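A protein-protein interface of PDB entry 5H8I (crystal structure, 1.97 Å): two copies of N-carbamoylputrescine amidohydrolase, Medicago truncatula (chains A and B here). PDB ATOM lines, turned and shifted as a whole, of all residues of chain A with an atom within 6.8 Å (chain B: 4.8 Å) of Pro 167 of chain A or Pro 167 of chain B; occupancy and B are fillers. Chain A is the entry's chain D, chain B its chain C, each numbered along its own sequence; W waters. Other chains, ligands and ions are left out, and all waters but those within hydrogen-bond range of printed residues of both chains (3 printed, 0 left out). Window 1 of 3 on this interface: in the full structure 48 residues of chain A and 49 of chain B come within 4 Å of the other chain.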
ATOM      1  N   ASP A 163      -2.766 -22.190  17.212  1.00  0.00           N
ATOM      2  CA  ASP A 163      -2.915 -22.931  15.950  1.00  0.00           C
ATOM      3  C   ASP A 163      -3.225 -22.042  14.726  1.00  0.00           C
ATOM      4  O   ASP A 163      -2.896 -22.416  13.587  1.00  0.00           O
ATOM      5  CB  ASP A 163      -4.061 -23.955  16.001  1.00  0.00           C
ATOM      6  CG  ASP A 163      -3.772 -25.197  16.846  1.00  0.00           C
ATOM      7  OD1 ASP A 163      -2.617 -25.634  16.921  1.00  0.00           O
ATOM      8  OD2 ASP A 163      -4.745 -25.775  17.408  1.00  0.00           O
ATOM      9  N   GLN A 164      -3.884 -20.885  14.969  1.00  0.00           N
ATOM     10  CA  GLN A 164      -4.304 -19.992  13.921  1.00  0.00           C
ATOM     11  C   GLN A 164      -3.119 -19.301  13.180  1.00  0.00           C
ATOM     12  O   GLN A 164      -3.325 -18.735  12.141  1.00  0.00           O
ATOM     13  CB  GLN A 164      -5.260 -18.926  14.502  1.00  0.00           C
ATOM     14  CG  GLN A 164      -4.561 -17.816  15.298  1.00  0.00           C
ATOM     15  CD  GLN A 164      -5.423 -17.257  16.423  1.00  0.00           C
ATOM     16  OE1 GLN A 164      -4.901 -16.827  17.470  1.00  0.00           O
ATOM     17  NE2 GLN A 164      -6.745 -17.270  16.229  1.00  0.00           N
ATOM     18  N   TRP A 165      -1.906 -19.355  13.746  1.00  0.00           N
ATOM     19  CA  TRP A 165      -0.727 -18.819  13.090  1.00  0.00           C
ATOM     20  C   TRP A 165      -0.131 -19.763  12.023  1.00  0.00           C
ATOM     21  O   TRP A 165       0.722 -19.340  11.304  1.00  0.00           O
ATOM     22  CB  TRP A 165       0.354 -18.458  14.134  1.00  0.00           C
ATOM     23  CG  TRP A 165      -0.106 -17.317  14.994  1.00  0.00           C
ATOM     24  CD1 TRP A 165      -0.880 -17.396  16.145  1.00  0.00           C
ATOM     25  CD2 TRP A 165       0.133 -15.925  14.773  1.00  0.00           C
ATOM     26  NE1 TRP A 165      -1.107 -16.123  16.633  1.00  0.00           N
ATOM     27  CE2 TRP A 165      -0.514 -15.212  15.826  1.00  0.00           C
ATOM     28  CE3 TRP A 165       0.842 -15.197  13.795  1.00  0.00           C
ATOM     29  CZ2 TRP A 165      -0.484 -13.808  15.919  1.00  0.00           C
ATOM     30  CZ3 TRP A 165       0.869 -13.801  13.883  1.00  0.00           C
ATOM     31  CH2 TRP A 165       0.219 -13.113  14.946  1.00  0.00           C
ATOM     32  N   PHE A 166      -0.603 -21.027  11.962  1.00  0.00           N
ATOM     33  CA  PHE A 166       0.025 -22.099  11.178  1.00  0.00           C
ATOM     34  C   PHE A 166      -0.745 -22.443   9.947  1.00  0.00           C
ATOM     35  O   PHE A 166      -1.795 -23.057  10.035  1.00  0.00           O
ATOM     36  CB  PHE A 166       0.224 -23.329  12.096  1.00  0.00           C
ATOM     37  CG  PHE A 166       1.175 -23.030  13.199  1.00  0.00           C
ATOM     38  CD1 PHE A 166       0.711 -22.445  14.402  1.00  0.00           C
ATOM     39  CD2 PHE A 166       2.517 -23.243  13.040  1.00  0.00           C
ATOM     40  CE1 PHE A 166       1.598 -22.118  15.416  1.00  0.00           C
ATOM     41  CE2 PHE A 166       3.398 -22.926  14.052  1.00  0.00           C
ATOM     42  CZ  PHE A 166       2.927 -22.360  15.232  1.00  0.00           C
ATOM     43  N   PRO A 167      -0.236 -22.039   8.759  1.00  0.00           N
ATOM     44  CA  PRO A 167      -0.951 -22.376   7.524  1.00  0.00           C
ATOM     45  C   PRO A 167      -1.163 -23.887   7.380  1.00  0.00           C
ATOM     46  O   PRO A 167      -2.144 -24.317   6.736  1.00  0.00           O
ATOM     47  CB  PRO A 167      -0.008 -21.879   6.426  1.00  0.00           C
ATOM     48  CG  PRO A 167       0.833 -20.844   7.058  1.00  0.00           C
ATOM     49  CD  PRO A 167       1.002 -21.279   8.492  1.00  0.00           C
ATOM     50  N   GLU A 168      -0.259 -24.688   7.965  1.00  0.00           N
ATOM     51  CA  GLU A 168      -0.421 -26.126   7.933  1.00  0.00           C
ATOM     52  C   GLU A 168      -1.729 -26.602   8.547  1.00  0.00           C
ATOM     53  O   GLU A 168      -2.338 -27.537   8.022  1.00  0.00           O
ATOM     54  CB  GLU A 168       0.738 -26.888   8.614  1.00  0.00           C
ATOM     55  CG  GLU A 168       2.126 -26.686   7.986  1.00  0.00           C
ATOM     56  CD  GLU A 168       2.943 -25.499   8.520  1.00  0.00           C
ATOM     57  OE1 GLU A 168       2.358 -24.508   9.042  1.00  0.00           O
ATOM     58  OE2 GLU A 168       4.171 -25.545   8.386  1.00  0.00           O
ATOM     59  N   ALA A 169      -2.177 -25.967   9.637  1.00  0.00           N
ATOM     60  CA  ALA A 169      -3.367 -26.407  10.313  1.00  0.00           C
ATOM     61  C   ALA A 169      -4.597 -26.132   9.462  1.00  0.00           C
ATOM     62  O   ALA A 169      -5.498 -26.995   9.339  1.00  0.00           O
ATOM     63  CB  ALA A 169      -3.497 -25.718  11.638  1.00  0.00           C
ATOM     64  N   ALA A 170      -4.624 -24.955   8.877  1.00  0.00           N
ATOM     65  CA  ALA A 170      -5.762 -24.546   8.015  1.00  0.00           C
ATOM     66  C   ALA A 170      -5.857 -25.430   6.767  1.00  0.00           C
ATOM     67  O   ALA A 170      -6.933 -25.905   6.398  1.00  0.00           O
ATOM     68  CB  ALA A 170      -5.623 -23.089   7.617  1.00  0.00           C
ATOM     69  N   ARG A 171      -4.718 -25.653   6.137  1.00  0.00           N
ATOM     70  CA  ARG A 171      -4.659 -26.541   4.964  1.00  0.00           C
ATOM     71  C   ARG A 171      -5.083 -27.972   5.327  1.00  0.00           C
ATOM     72  O   ARG A 171      -5.820 -28.588   4.596  1.00  0.00           O
ATOM     73  CB  ARG A 171      -3.261 -26.562   4.357  1.00  0.00           C
ATOM     74  CG  ARG A 171      -3.186 -27.403   3.085  1.00  0.00           C
ATOM     75  CD  ARG A 171      -3.923 -26.679   1.953  1.00  0.00           C
ATOM     76  NE  ARG A 171      -3.039 -25.990   1.047  1.00  0.00           N
ATOM     77  CZ  ARG A 171      -3.416 -25.066   0.201  1.00  0.00           C
ATOM     78  NH1 ARG A 171      -4.683 -24.624   0.201  1.00  0.00           N
ATOM     79  NH2 ARG A 171      -2.530 -24.535  -0.642  1.00  0.00           N
ATOM     80  N   ALA A 172      -4.610 -28.476   6.454  1.00  0.00           N
ATOM     81  CA  ALA A 172      -4.930 -29.824   6.877  1.00  0.00           C
ATOM     82  C   ALA A 172      -6.427 -30.011   7.039  1.00  0.00           C
ATOM     83  O   ALA A 172      -6.983 -31.033   6.634  1.00  0.00           O
ATOM     84  CB  ALA A 172      -4.213 -30.132   8.176  1.00  0.00           C
ATOM     85  N   TYR A 183     -11.519 -20.484  15.086  1.00  0.00           N
ATOM     86  CA  TYR A 183     -10.420 -20.373  16.031  1.00  0.00           C
ATOM     87  C   TYR A 183     -10.760 -19.547  17.320  1.00  0.00           C
ATOM     88  O   TYR A 183     -10.673 -18.310  17.319  1.00  0.00           O
ATOM     89  CB  TYR A 183      -9.238 -19.714  15.365  1.00  0.00           C
ATOM     90  CG  TYR A 183      -8.641 -20.421  14.168  1.00  0.00           C
ATOM     91  CD1 TYR A 183      -7.614 -21.339  14.315  1.00  0.00           C
ATOM     92  CD2 TYR A 183      -9.088 -20.156  12.870  1.00  0.00           C
ATOM     93  CE1 TYR A 183      -7.050 -21.985  13.197  1.00  0.00           C
ATOM     94  CE2 TYR A 183      -8.523 -20.821  11.759  1.00  0.00           C
ATOM     95  CZ  TYR A 183      -7.515 -21.715  11.930  1.00  0.00           C
ATOM     96  OH  TYR A 183      -6.935 -22.361  10.876  1.00  0.00           O
ATOM     97  N   VAL A 205      -2.484 -12.983   9.030  1.00  0.00           N
ATOM     98  CA  VAL A 205      -2.124 -14.398   8.896  1.00  0.00           C
ATOM     99  C   VAL A 205      -3.380 -15.249   8.703  1.00  0.00           C
ATOM    100  O   VAL A 205      -3.409 -16.127   7.841  1.00  0.00           O
ATOM    101  CB  VAL A 205      -1.231 -14.842  10.083  1.00  0.00           C
ATOM    102  CG1 VAL A 205      -1.030 -16.335  10.096  1.00  0.00           C
ATOM    103  CG2 VAL A 205       0.126 -14.153   9.973  1.00  0.00           C
ATOM    104  N   GLY A 208      -4.967 -14.740   5.328  1.00  0.00           N
ATOM    105  CA  GLY A 208      -4.177 -15.590   4.419  1.00  0.00           C
ATOM    106  C   GLY A 208      -4.675 -17.020   4.306  1.00  0.00           C
ATOM    107  O   GLY A 208      -4.778 -17.531   3.196  1.00  0.00           O
ATOM    108  N   HIS A 209      -4.996 -17.643   5.430  1.00  0.00           N
ATOM    109  CA  HIS A 209      -5.529 -18.981   5.434  1.00  0.00           C
ATOM    110  C   HIS A 209      -6.877 -19.061   4.738  1.00  0.00           C
ATOM    111  O   HIS A 209      -7.115 -19.994   3.963  1.00  0.00           O
ATOM    112  CB  HIS A 209      -5.770 -19.547   6.825  1.00  0.00           C
ATOM    113  CG  HIS A 209      -4.616 -19.460   7.763  1.00  0.00           C
ATOM    114  ND1 HIS A 209      -3.286 -19.423   7.352  1.00  0.00           N
ATOM    115  CD2 HIS A 209      -4.599 -19.436   9.122  1.00  0.00           C
ATOM    116  CE1 HIS A 209      -2.507 -19.361   8.431  1.00  0.00           C
ATOM    117  NE2 HIS A 209      -3.280 -19.374   9.512  1.00  0.00           N
ATOM    118  N   ALA A 212      -6.237 -18.671   0.992  1.00  0.00           N
ATOM    119  CA  ALA A 212      -5.442 -19.721   0.375  1.00  0.00           C
ATOM    120  C   ALA A 212      -6.219 -20.996   0.231  1.00  0.00           C
ATOM    121  O   ALA A 212      -5.958 -21.785  -0.680  1.00  0.00           O
ATOM    122  CB  ALA A 212      -4.177 -19.960   1.123  1.00  0.00           C
ATOM    123  N   ASN A 213      -7.183 -21.202   1.109  1.00  0.00           N
ATOM    124  CA  ASN A 213      -8.023 -22.402   1.084  1.00  0.00           C
ATOM    125  C   ASN A 213      -9.424 -22.158   0.526  1.00  0.00           C
ATOM    126  O   ASN A 213     -10.192 -23.124   0.290  1.00  0.00           O
ATOM    127  CB  ASN A 213      -8.116 -22.963   2.477  1.00  0.00           C
ATOM    128  CG  ASN A 213      -6.790 -23.503   2.972  1.00  0.00           C
ATOM    129  OD1 ASN A 213      -6.345 -24.582   2.550  1.00  0.00           O
ATOM    130  ND2 ASN A 213      -6.139 -22.765   3.847  1.00  0.00           N
ATOM    131  N   LEU A 294       8.179 -29.985   4.464  1.00  0.00           N
ATOM    132  CA  LEU A 294       7.261 -29.578   5.504  1.00  0.00           C
ATOM    133  C   LEU A 294       7.224 -30.540   6.688  1.00  0.00           C
ATOM    134  O   LEU A 294       6.757 -30.157   7.755  1.00  0.00           O
ATOM    135  CB  LEU A 294       5.840 -29.371   4.997  1.00  0.00           C
ATOM    136  CG  LEU A 294       5.708 -28.402   3.809  1.00  0.00           C
ATOM    137  CD1 LEU A 294       4.255 -28.266   3.456  1.00  0.00           C
ATOM    138  CD2 LEU A 294       6.291 -27.066   4.101  1.00  0.00           C
ATOM    139  N   TRP B 165       0.243 -18.520  -4.498  1.00  0.00           N
ATOM    140  CA  TRP B 165      -1.000 -18.809  -3.815  1.00  0.00           C
ATOM    141  C   TRP B 165      -0.872 -19.954  -2.790  1.00  0.00           C
ATOM    142  O   TRP B 165      -1.841 -20.232  -2.059  1.00  0.00           O
ATOM    143  CB  TRP B 165      -2.075 -19.177  -4.840  1.00  0.00           C
ATOM    144  CG  TRP B 165      -2.450 -17.997  -5.707  1.00  0.00           C
ATOM    145  CD1 TRP B 165      -1.813 -17.588  -6.836  1.00  0.00           C
ATOM    146  CD2 TRP B 165      -3.531 -17.072  -5.490  1.00  0.00           C
ATOM    147  NE1 TRP B 165      -2.439 -16.466  -7.350  1.00  0.00           N
ATOM    148  CE2 TRP B 165      -3.494 -16.128  -6.543  1.00  0.00           C
ATOM    149  CE3 TRP B 165      -4.534 -16.956  -4.518  1.00  0.00           C
ATOM    150  CZ2 TRP B 165      -4.404 -15.102  -6.658  1.00  0.00           C
ATOM    151  CZ3 TRP B 165      -5.446 -15.908  -4.629  1.00  0.00           C
ATOM    152  CH2 TRP B 165      -5.379 -14.993  -5.704  1.00  0.00           C
ATOM    153  N   PHE B 166       0.313 -20.621  -2.746  1.00  0.00           N
ATOM    154  CA  PHE B 166       0.470 -21.861  -1.982  1.00  0.00           C
ATOM    155  C   PHE B 166       1.297 -21.596  -0.739  1.00  0.00           C
ATOM    156  O   PHE B 166       2.501 -21.316  -0.830  1.00  0.00           O
ATOM    157  CB  PHE B 166       1.081 -22.917  -2.871  1.00  0.00           C
ATOM    158  CG  PHE B 166       0.183 -23.284  -3.973  1.00  0.00           C
ATOM    159  CD1 PHE B 166       0.171 -22.537  -5.139  1.00  0.00           C
ATOM    160  CD2 PHE B 166      -0.688 -24.353  -3.835  1.00  0.00           C
ATOM    161  CE1 PHE B 166      -0.698 -22.846  -6.191  1.00  0.00           C
ATOM    162  CE2 PHE B 166      -1.558 -24.684  -4.875  1.00  0.00           C
ATOM    163  CZ  PHE B 166      -1.563 -23.922  -6.041  1.00  0.00           C
ATOM    164  N   PRO B 167       0.661 -21.682   0.441  1.00  0.00           N
ATOM    165  CA  PRO B 167       1.467 -21.542   1.657  1.00  0.00           C
ATOM    166  C   PRO B 167       2.581 -22.517   1.781  1.00  0.00           C
ATOM    167  O   PRO B 167       3.594 -22.194   2.400  1.00  0.00           O
ATOM    168  CB  PRO B 167       0.439 -21.766   2.780  1.00  0.00           C
ATOM    169  CG  PRO B 167      -0.849 -21.349   2.173  1.00  0.00           C
ATOM    170  CD  PRO B 167      -0.753 -21.860   0.765  1.00  0.00           C
ATOM    171  N   GLU B 168       2.409 -23.708   1.205  1.00  0.00           N
ATOM    172  CA  GLU B 168       3.423 -24.745   1.244  1.00  0.00           C
ATOM    173  C   GLU B 168       4.763 -24.297   0.644  1.00  0.00           C
ATOM    174  O   GLU B 168       5.840 -24.652   1.136  1.00  0.00           O
ATOM    175  CB  GLU B 168       2.931 -26.012   0.506  1.00  0.00           C
ATOM    176  CG  GLU B 168       1.807 -26.717   1.179  1.00  0.00           C
ATOM    177  CD  GLU B 168       0.421 -26.301   0.668  1.00  0.00           C
ATOM    178  OE1 GLU B 168       0.260 -25.134   0.188  1.00  0.00           O
ATOM    179  OE2 GLU B 168      -0.503 -27.138   0.762  1.00  0.00           O
ATOM    180  N   ALA B 169       4.684 -23.503  -0.428  1.00  0.00           N
ATOM    181  CA  ALA B 169       5.885 -23.057  -1.142  1.00  0.00           C
ATOM    182  C   ALA B 169       6.651 -22.036  -0.290  1.00  0.00           C
ATOM    183  O   ALA B 169       7.863 -22.132  -0.156  1.00  0.00           O
ATOM    184  CB  ALA B 169       5.498 -22.449  -2.457  1.00  0.00           C
ATOM    185  N   ALA B 170       5.919 -21.076   0.270  1.00  0.00           N
ATOM    186  CA  ALA B 170       6.518 -20.064   1.119  1.00  0.00           C
ATOM    187  C   ALA B 170       7.149 -20.728   2.356  1.00  0.00           C
ATOM    188  O   ALA B 170       8.281 -20.417   2.702  1.00  0.00           O
ATOM    189  CB  ALA B 170       5.510 -19.040   1.528  1.00  0.00           C
ATOM    190  N   ARG B 171       6.418 -21.637   2.996  1.00  0.00           N
ATOM    191  CA  ARG B 171       6.960 -22.345   4.144  1.00  0.00           C
ATOM    192  C   ARG B 171       8.189 -23.210   3.771  1.00  0.00           C
ATOM    193  O   ARG B 171       9.176 -23.228   4.494  1.00  0.00           O
ATOM    194  CB  ARG B 171       5.893 -23.236   4.789  1.00  0.00           C
ATOM    195  CG  ARG B 171       6.380 -23.957   6.040  1.00  0.00           C
ATOM    196  CD  ARG B 171       6.535 -22.959   7.185  1.00  0.00           C
ATOM    197  NE  ARG B 171       5.415 -23.019   8.101  1.00  0.00           N
ATOM    198  CZ  ARG B 171       5.107 -22.071   8.967  1.00  0.00           C
ATOM    199  NH1 ARG B 171       5.787 -20.959   8.993  1.00  0.00           N
ATOM    200  NH2 ARG B 171       4.108 -22.239   9.795  1.00  0.00           N
ATOM    201  N   HIS B 209       1.540 -15.215   3.841  1.00  0.00           N
ATOM    202  CA  HIS B 209       2.835 -15.969   3.801  1.00  0.00           C
ATOM    203  C   HIS B 209       3.923 -15.202   4.540  1.00  0.00           C
ATOM    204  O   HIS B 209       4.682 -15.769   5.315  1.00  0.00           O
ATOM    205  CB  HIS B 209       3.400 -16.225   2.388  1.00  0.00           C
ATOM    206  CG  HIS B 209       2.465 -16.894   1.449  1.00  0.00           C
ATOM    207  ND1 HIS B 209       1.479 -17.763   1.862  1.00  0.00           N
ATOM    208  CD2 HIS B 209       2.379 -16.839   0.099  1.00  0.00           C
ATOM    209  CE1 HIS B 209       0.814 -18.196   0.809  1.00  0.00           C
ATOM    210  NE2 HIS B 209       1.339 -17.643  -0.272  1.00  0.00           N
ATOM    211  N   ALA B 212       3.195 -15.326   8.301  1.00  0.00           N
ATOM    212  CA  ALA B 212       3.261 -16.640   8.902  1.00  0.00           C
ATOM    213  C   ALA B 212       4.674 -17.157   9.008  1.00  0.00           C
ATOM    214  O   ALA B 212       4.988 -17.969   9.885  1.00  0.00           O
ATOM    215  CB  ALA B 212       2.427 -17.624   8.098  1.00  0.00           C
HETATM  216  O   HOH W   1      -3.507 -22.229  -1.971  1.00  0.00           O
HETATM  217  O   HOH W   2      -1.833 -17.428   2.878  1.00  0.00           O
HETATM  218  O   HOH W   3       3.476 -19.837  11.141  1.00  0.00           O
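The guanidinium group (NE) of Arg 171 of chain A is in salt-bridge range of the side-chain carboxylate (OE2) of Glu 168 of chain B, at 2.8 Å. The side-chain carboxylate of Glu 168 of chain A is in salt-bridge range of the guanidinium group of Arg 171 of chain B.
O of Val 205 of chain A sits at hydrogen-bond distance from ND1 of His 209 of chain A. The backbone carbonyl oxygen of Ala 212 of chain B lies within hydrogen-bond range of the guanidinium group of Arg 171 of chain B, at 3.2 Å. The guanidinium group (NH1) of Arg 171 of chain A sits at hydrogen-bond distance from the backbone carbonyl oxygen (O) of Ala 212 of chain A. The guanidinium group (NH1) of Arg 171 of chain A lies within hydrogen-bond range of the side-chain amide oxygen (OD1) of Asn 213 of chain A.
Among the printed residues, merely in contact across the chains: Pro 167 of chain A with Arg 171 of chain B (3.5 Å), Arg 171 of chain A with Pro 167 of chain B (3.5 Å), Leu 294 of chain A with Arg 171 of chain B (3.7 Å), Pro 167 of chain A with Pro 167 of chain B (3.7 Å), Leu 294 of chain A with Glu 168 of chain B (3.7 Å), Val 205 of chain A with Ala 212 of chain B (3.7 Å), Arg 171 of chain A with Phe 166 of chain B (3.7 Å), Pro 167 of chain A with Ala 212 of chain B (3.7 Å), Phe 166 of chain A with Arg 171 of chain B (3.8 Å), Ala 212 of chain A with Pro 167 of chain B (3.8 Å) and Ala 212 of chain A with Trp 165 of chain B (3.96 Å).
Pro 167 of chain A touches just these residues of chain B: Pro 167, Arg 171 and Ala 212. Ala 170 of chain A touches none of the printed residues of chain B. Printed residues of chain B within 4 Å of Arg 171 of chain A: Phe 166 (3.7 Å), Pro 167 (3.5 Å) and Glu 168 (2.8 Å). Of the printed residues of chain B, Val 205 of chain A touches Ala 212 (3.7 Å). Of chain A, only Pro 167, Arg 171 and Ala 212 come within 4 Å of Pro 167 of chain B. Ala 169 of chain B touches none of the printed residues of chain A.
Of the 17 printed residues of chain A, 7 touch a printed residue of chain B. Hydrophobic or aromatic side chains of chain A within 4 Å of the printed part of chain B: Phe 166, Pro 167, Val 205, Ala 212 and Leu 294. Printed residues of chain B that touch a printed residue of chain A: Trp 165, Phe 166, Pro 167, Glu 168, Arg 171 and Ala 212. Hydrophobic or aromatic side chains of chain B that line the printed part of chain A: Phe 166, Pro 167 and Ala 212. Among the printed residues, Asp or Glu carboxylates within 4 Å of a Lys or Arg side-chain nitrogen of the other chain: Glu 168 of chain A with Arg 171 of chain B and Arg 171 of chain A with Glu 168 of chain B.
Pro 167 of chain A touches Arg 171 of chain B, and with the chains exchanged Arg 171 of chain A touches Pro 167 of chain B. Pro 167 of chain A touches Ala 212 of chain B, and with the chains exchanged Ala 212 of chain A touches Pro 167 of chain B. Glu 168 of chain A touches Arg 171 of chain B, and with the chains exchanged Arg 171 of chain A touches Glu 168 of chain B. Ala 212 of chain A touches Trp 165 of chain B, but with the chains exchanged Trp 165 of chain A does not touch Ala 212 of chain B (4.02 Å). Positions printed for both chains: 165, 166, 167, 168, 169, 170, 171, 209 and 212. Of the 13 pairs that touch across the chains among the printed residues, 9 have their exchanged pair printed and touching as well.
Water W1 lies within hydrogen-bond range of O of Trp 165 of chain B (2.6 Å), O of Ala 212 of chain A (2.8 Å) and NH2 of Arg 171 of chain A (2.8 Å). Water W3 lies within hydrogen-bond range of the backbone carbonyl oxygen of Ala 212 of chain B (2.7 Å), the backbone carbonyl oxygen of Trp 165 of chain A (2.8 Å) and the guanidinium group of Arg 171 of chain B (2.8 Å). Water W2 lies within hydrogen-bond range of O of Gly 208 of chain A (3.0 Å) and ND1 of His 209 of chain B (3.5 Å).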
